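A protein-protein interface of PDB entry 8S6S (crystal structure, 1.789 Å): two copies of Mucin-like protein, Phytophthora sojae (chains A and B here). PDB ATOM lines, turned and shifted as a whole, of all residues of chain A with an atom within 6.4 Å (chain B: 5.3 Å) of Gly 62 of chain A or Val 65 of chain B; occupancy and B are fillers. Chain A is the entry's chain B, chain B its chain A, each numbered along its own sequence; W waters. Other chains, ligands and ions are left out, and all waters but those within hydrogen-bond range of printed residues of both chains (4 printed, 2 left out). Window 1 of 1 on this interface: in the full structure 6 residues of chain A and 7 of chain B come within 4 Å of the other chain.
Leu 59 of chain A touches none of the printed residues of chain B.
Gly 62 of chain A touches just these residues of chain B: Glu 24 (3.6 Å), Gln 26 (2.9 Å) and Val 65 (3.8 Å).
Of the printed residues of chain B, Pro 64 of chain A touches Glu 24 (3.5 Å) and Gln 26 (3.9 Å).
Of the printed residues of chain B, Asp 69 of chain A touches Asn 63.
Of the printed residues of chain A, Asn 63 of chain B touches Asp 69 (3.0 Å).
The nearest residue of chain A that does not touch Val 65 of chain B is Asp 61 of chain A (4.1 Å).
The nearest printed residue of chain B that does not touch Pro 64 of chain A is Ile 23 of chain B (7.8 Å).
Printed residues of chain B that touch a printed residue of chain A: Glu 24, Gln 26, Asn 63, Pro 64 and Val 65.
Hydrophobic or aromatic side chains of chain B within 4 Å of the printed part of chain A: Pro 64 and Val 65.
Of the 9 printed residues of chain A, 5 touch a printed residue of chain B.
Printed residues of chain A that touch a printed residue of chain B: Arg 57, Gly 62, Asn 63, Pro 64 and Asp 69.
Hydrophobic or aromatic side chains of chain A that line the printed part of chain B: Pro 64.
Along chain A the printed residues that touch a printed residue of chain B span positions 57 to 69.
Among the printed residues, no Asp or Glu carboxylate lies within 4 Å of a Lys or Arg side-chain nitrogen of the other chain.
Water W2 lies within hydrogen-bond range of OE1 of Glu 24 of chain B and O of Gly 62 of chain A.
Water W3 lies within hydrogen-bond range of OD2 of Asp 69 of chain A (2.6 Å) and OE1 of Gln 26 of chain B (2.7 Å).
Water W1 lies within hydrogen-bond range of OD1 of Asn 63 of chain A and OE2 of Glu 24 of chain B.
Water W4 lies within hydrogen-bond range of N of Glu 24 of chain B (3.0 Å) and O of Gly 62 of chain A (3.2 Å).
Positions printed for both chains: 63 and 64.
Of the 8 pairs that touch across the chains among the printed residues, none has its exchanged pair printed and touching as well.
NH2 of Arg 57 of chain A touches CG of Pro 64 of chain B (3.5 Å).
Glu 24 of chain B touches Gly 62 of chain A (CG to O, 3.6 Å).
Gly 62 of chain A touches Val 65 of chain B (N to CG1, 3.8 Å).
OE1 of Glu 24 of chain B touches CG of Asn 63 of chain A (3.8 Å).
Pro 64 of chain A touches Glu 24 of chain B.
Pro 64 of chain A touches Gln 26 of chain B (CG to O, 3.9 Å).
The side-chain carboxylate (OD2) of Asp 69 of chain A lies within hydrogen-bond range of the side-chain amide nitrogen (ND2) of Asn 63 of chain B (3.0 Å).
The side-chain amide nitrogen of Gln 26 of chain B sits at hydrogen-bond distance from the backbone carbonyl oxygen of Gly 62 of chain A (2.9 Å).
The backbone carbonyl oxygen (O) of Glu 24 of chain B is in hydrogen-bond range of the side-chain amide nitrogen (NE2) of Gln 26 of chain B.
OD1 of Asn 63 of chain B is in hydrogen-bond range of N of Val 65 of chain B (3.0 Å).
NE of Arg 57 of chain A is in salt-bridge range of OD2 of Asp 61 of chain A (2.9 Å).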
ATOM      1  N   ARG A  57     -35.262  -2.965  26.298  1.00  0.00           N
ATOM      2  CA  ARG A  57     -33.855  -2.545  26.251  1.00  0.00           C
ATOM      3  C   ARG A  57     -33.633  -1.578  25.087  1.00  0.00           C
ATOM      4  O   ARG A  57     -33.000  -0.541  25.259  1.00  0.00           O
ATOM      5  CB  ARG A  57     -32.913  -3.748  26.183  1.00  0.00           C
ATOM      6  CG  ARG A  57     -31.470  -3.305  25.978  1.00  0.00           C
ATOM      7  CD  ARG A  57     -30.522  -4.493  25.991  1.00  0.00           C
ATOM      8  NE  ARG A  57     -29.162  -3.978  26.175  1.00  0.00           N
ATOM      9  CZ  ARG A  57     -28.119  -4.779  26.251  1.00  0.00           C
ATOM     10  NH1 ARG A  57     -28.297  -6.081  26.085  1.00  0.00           N
ATOM     11  NH2 ARG A  57     -26.923  -4.264  26.491  1.00  0.00           N
ATOM     12  N   SER A  58     -34.186  -1.862  23.902  1.00  0.00           N
ATOM     13  CA  SER A  58     -33.996  -1.025  22.730  1.00  0.00           C
ATOM     14  C   SER A  58     -34.693   0.312  22.936  1.00  0.00           C
ATOM     15  O   SER A  58     -34.274   1.304  22.366  1.00  0.00           O
ATOM     16  CB  SER A  58     -34.547  -1.668  21.447  1.00  0.00           C
ATOM     17  OG  SER A  58     -33.944  -2.915  21.220  1.00  0.00           O
ATOM     18  N   LEU A  59     -35.792   0.310  23.688  1.00  0.00           N
ATOM     19  CA  LEU A  59     -36.504   1.533  24.002  1.00  0.00           C
ATOM     20  C   LEU A  59     -35.694   2.440  24.931  1.00  0.00           C
ATOM     21  O   LEU A  59     -35.580   3.633  24.636  1.00  0.00           O
ATOM     22  CB  LEU A  59     -37.878   1.197  24.599  1.00  0.00           C
ATOM     23  CG  LEU A  59     -38.685   2.418  25.014  1.00  0.00           C
ATOM     24  CD1 LEU A  59     -39.186   3.156  23.786  1.00  0.00           C
ATOM     25  CD2 LEU A  59     -39.856   2.016  25.902  1.00  0.00           C
ATOM     26  N   MET A  60     -35.088   1.886  25.996  1.00  0.00           N
ATOM     27  CA  MET A  60     -34.447   2.652  27.070  1.00  0.00           C
ATOM     28  C   MET A  60     -32.993   3.020  26.754  1.00  0.00           C
ATOM     29  O   MET A  60     -32.574   4.170  26.953  1.00  0.00           O
ATOM     30  CB  MET A  60     -34.467   1.838  28.367  1.00  0.00           C
ATOM     31  CG  MET A  60     -35.891   1.678  28.896  1.00  0.00           C
ATOM     32  SD  MET A  60     -35.826   1.178  30.571  1.00  0.00           S
ATOM     33  CE  MET A  60     -37.579   0.942  30.902  1.00  0.00           C
ATOM     34  N   ASP A  61     -32.246   2.065  26.197  1.00  0.00           N
ATOM     35  CA  ASP A  61     -30.795   2.262  26.024  1.00  0.00           C
ATOM     36  C   ASP A  61     -30.529   3.441  25.097  1.00  0.00           C
ATOM     37  O   ASP A  61     -31.034   3.493  23.974  1.00  0.00           O
ATOM     38  CB  ASP A  61     -30.088   1.045  25.415  1.00  0.00           C
ATOM     39  CG  ASP A  61     -29.709  -0.070  26.385  1.00  0.00           C
ATOM     40  OD1 ASP A  61     -30.036   0.037  27.604  1.00  0.00           O
ATOM     41  OD2 ASP A  61     -29.117  -1.097  25.883  1.00  0.00           O
ATOM     42  N   GLY A  62     -29.707   4.399  25.567  1.00  0.00           N
ATOM     43  CA  GLY A  62     -29.324   5.490  24.700  1.00  0.00           C
ATOM     44  C   GLY A  62     -30.270   6.678  24.755  1.00  0.00           C
ATOM     45  O   GLY A  62     -29.984   7.688  24.129  1.00  0.00           O
ATOM     46  N   ASN A  63     -31.404   6.562  25.474  1.00  0.00           N
ATOM     47  CA  ASN A  63     -32.329   7.670  25.585  1.00  0.00           C
ATOM     48  C   ASN A  63     -32.347   8.156  27.019  1.00  0.00           C
ATOM     49  O   ASN A  63     -32.842   7.474  27.921  1.00  0.00           O
ATOM     50  CB  ASN A  63     -33.728   7.271  25.116  1.00  0.00           C
ATOM     51  CG  ASN A  63     -34.670   8.452  25.138  1.00  0.00           C
ATOM     52  OD1 ASN A  63     -34.399   9.465  25.803  1.00  0.00           O
ATOM     53  ND2 ASN A  63     -35.796   8.308  24.447  1.00  0.00           N
ATOM     54  N   PRO A  64     -31.752   9.333  27.316  1.00  0.00           N
ATOM     55  CA  PRO A  64     -31.639   9.803  28.690  1.00  0.00           C
ATOM     56  C   PRO A  64     -32.943  10.054  29.444  1.00  0.00           C
ATOM     57  O   PRO A  64     -32.891  10.161  30.645  1.00  0.00           O
ATOM     58  CB  PRO A  64     -30.828  11.114  28.630  1.00  0.00           C
ATOM     59  CG  PRO A  64     -30.374  11.235  27.216  1.00  0.00           C
ATOM     60  CD  PRO A  64     -31.121  10.247  26.348  1.00  0.00           C
ATOM     61  N   ASP A  69     -27.887   4.629  32.805  1.00  0.00           N
ATOM     62  CA  ASP A  69     -27.674   3.201  32.595  1.00  0.00           C
ATOM     63  C   ASP A  69     -27.473   2.510  33.941  1.00  0.00           C
ATOM     64  O   ASP A  69     -26.919   3.118  34.847  1.00  0.00           O
ATOM     65  CB  ASP A  69     -26.455   2.957  31.706  1.00  0.00           C
ATOM     66  CG  ASP A  69     -26.675   3.391  30.264  1.00  0.00           C
ATOM     67  OD1 ASP A  69     -27.632   2.887  29.579  1.00  0.00           O
ATOM     68  OD2 ASP A  69     -25.863   4.190  29.805  1.00  0.00           O
ATOM     69  N   VAL B  21     -21.092   4.560  16.194  1.00  0.00           N
ATOM     70  CA  VAL B  21     -22.487   4.932  16.430  1.00  0.00           C
ATOM     71  C   VAL B  21     -22.648   6.447  16.379  1.00  0.00           C
ATOM     72  O   VAL B  21     -21.681   7.165  16.570  1.00  0.00           O
ATOM     73  CB  VAL B  21     -22.989   4.397  17.771  1.00  0.00           C
ATOM     74  CG1 VAL B  21     -23.003   2.884  17.805  1.00  0.00           C
ATOM     75  CG2 VAL B  21     -22.276   4.996  18.974  1.00  0.00           C
ATOM     76  N   ILE B  23     -25.461   9.007  18.255  1.00  0.00           N
ATOM     77  CA  ILE B  23     -26.497   8.916  19.271  1.00  0.00           C
ATOM     78  C   ILE B  23     -26.845  10.310  19.768  1.00  0.00           C
ATOM     79  O   ILE B  23     -26.104  11.267  19.591  1.00  0.00           O
ATOM     80  CB  ILE B  23     -26.056   8.003  20.438  1.00  0.00           C
ATOM     81  CG1 ILE B  23     -24.780   8.539  21.108  1.00  0.00           C
ATOM     82  CG2 ILE B  23     -25.921   6.531  19.995  1.00  0.00           C
ATOM     83  CD1 ILE B  23     -24.264   7.652  22.165  1.00  0.00           C
ATOM     84  N   GLU B  24     -27.998  10.418  20.447  1.00  0.00           N
ATOM     85  CA  GLU B  24     -28.274  11.679  21.095  1.00  0.00           C
ATOM     86  C   GLU B  24     -27.293  11.840  22.261  1.00  0.00           C
ATOM     87  O   GLU B  24     -26.695  10.904  22.780  1.00  0.00           O
ATOM     88  CB  GLU B  24     -29.728  11.789  21.559  1.00  0.00           C
ATOM     89  CG  GLU B  24     -30.072  10.969  22.741  1.00  0.00           C
ATOM     90  CD  GLU B  24     -31.578  11.093  22.990  1.00  0.00           C
ATOM     91  OE1 GLU B  24     -32.316  10.137  22.678  1.00  0.00           O
ATOM     92  OE2 GLU B  24     -32.013  12.169  23.451  1.00  0.00           O
ATOM     93  N   GLN B  26     -25.794  11.811  25.713  1.00  0.00           N
ATOM     94  CA  GLN B  26     -26.227  10.872  26.736  1.00  0.00           C
ATOM     95  C   GLN B  26     -26.443  11.576  28.066  1.00  0.00           C
ATOM     96  O   GLN B  26     -26.935  10.966  29.010  1.00  0.00           O
ATOM     97  CB  GLN B  26     -25.233   9.715  26.890  1.00  0.00           C
ATOM     98  CG  GLN B  26     -25.167   8.863  25.653  1.00  0.00           C
ATOM     99  CD  GLN B  26     -26.500   8.165  25.449  1.00  0.00           C
ATOM    100  OE1 GLN B  26     -26.920   7.291  26.224  1.00  0.00           O
ATOM    101  NE2 GLN B  26     -27.220   8.604  24.440  1.00  0.00           N
ATOM    102  N   ASN B  63     -20.298  -0.495  27.594  1.00  0.00           N
ATOM    103  CA  ASN B  63     -21.616   0.095  27.408  1.00  0.00           C
ATOM    104  C   ASN B  63     -21.973  -0.035  25.945  1.00  0.00           C
ATOM    105  O   ASN B  63     -21.480   0.696  25.078  1.00  0.00           O
ATOM    106  CB  ASN B  63     -21.710   1.526  27.936  1.00  0.00           C
ATOM    107  CG  ASN B  63     -23.119   2.087  27.817  1.00  0.00           C
ATOM    108  OD1 ASN B  63     -23.971   1.545  27.122  1.00  0.00           O
ATOM    109  ND2 ASN B  63     -23.338   3.207  28.464  1.00  0.00           N
ATOM    110  N   PRO B  64     -22.874  -0.978  25.593  1.00  0.00           N
ATOM    111  CA  PRO B  64     -23.284  -1.191  24.205  1.00  0.00           C
ATOM    112  C   PRO B  64     -23.903  -0.015  23.464  1.00  0.00           C
ATOM    113  O   PRO B  64     -23.957  -0.005  22.239  1.00  0.00           O
ATOM    114  CB  PRO B  64     -24.339  -2.288  24.378  1.00  0.00           C
ATOM    115  CG  PRO B  64     -23.811  -3.052  25.541  1.00  0.00           C
ATOM    116  CD  PRO B  64     -23.476  -1.954  26.515  1.00  0.00           C
ATOM    117  N   VAL B  65     -24.349   1.012  24.197  1.00  0.00           N
ATOM    118  CA  VAL B  65     -24.851   2.170  23.484  1.00  0.00           C
ATOM    119  C   VAL B  65     -23.752   2.796  22.622  1.00  0.00           C
ATOM    120  O   VAL B  65     -24.078   3.380  21.605  1.00  0.00           O
ATOM    121  CB  VAL B  65     -25.708   3.197  24.255  1.00  0.00           C
ATOM    122  CG1 VAL B  65     -26.351   2.703  25.546  1.00  0.00           C
ATOM    123  CG2 VAL B  65     -25.123   4.567  24.384  1.00  0.00           C
ATOM    124  N   TYR B  66     -22.487   2.589  22.982  1.00  0.00           N
ATOM    125  CA  TYR B  66     -21.391   3.119  22.164  1.00  0.00           C
ATOM    126  C   TYR B  66     -20.892   2.150  21.102  1.00  0.00           C
ATOM    127  O   TYR B  66     -19.892   2.440  20.434  1.00  0.00           O
ATOM    128  CB  TYR B  66     -20.292   3.553  23.133  1.00  0.00           C
ATOM    129  CG  TYR B  66     -20.693   4.723  24.017  1.00  0.00           C
ATOM    130  CD1 TYR B  66     -20.670   6.029  23.547  1.00  0.00           C
ATOM    131  CD2 TYR B  66     -21.153   4.509  25.301  1.00  0.00           C
ATOM    132  CE1 TYR B  66     -21.084   7.070  24.344  1.00  0.00           C
ATOM    133  CE2 TYR B  66     -21.619   5.551  26.094  1.00  0.00           C
ATOM    134  CZ  TYR B  66     -21.568   6.843  25.608  1.00  0.00           C
ATOM    135  OH  TYR B  66     -21.967   7.839  26.451  1.00  0.00           O
ATOM    136  N   GLY B  67     -21.610   1.037  20.898  1.00  0.00           N
ATOM    137  CA  GLY B  67     -21.389   0.160  19.753  1.00  0.00           C
ATOM    138  C   GLY B  67     -20.268  -0.846  19.995  1.00  0.00           C
ATOM    139  O   GLY B  67     -19.716  -0.915  21.073  1.00  0.00           O
HETATM  140  O   HOH W   1     -34.226  11.984  24.984  1.00  0.00           O
HETATM  141  O   HOH W   2     -31.991   7.834  21.674  1.00  0.00           O
HETATM  142  O   HOH W   3     -25.482   6.159  28.190  1.00  0.00           O
HETATM  143  O   HOH W   4     -29.512   7.905  20.953  1.00  0.00           O
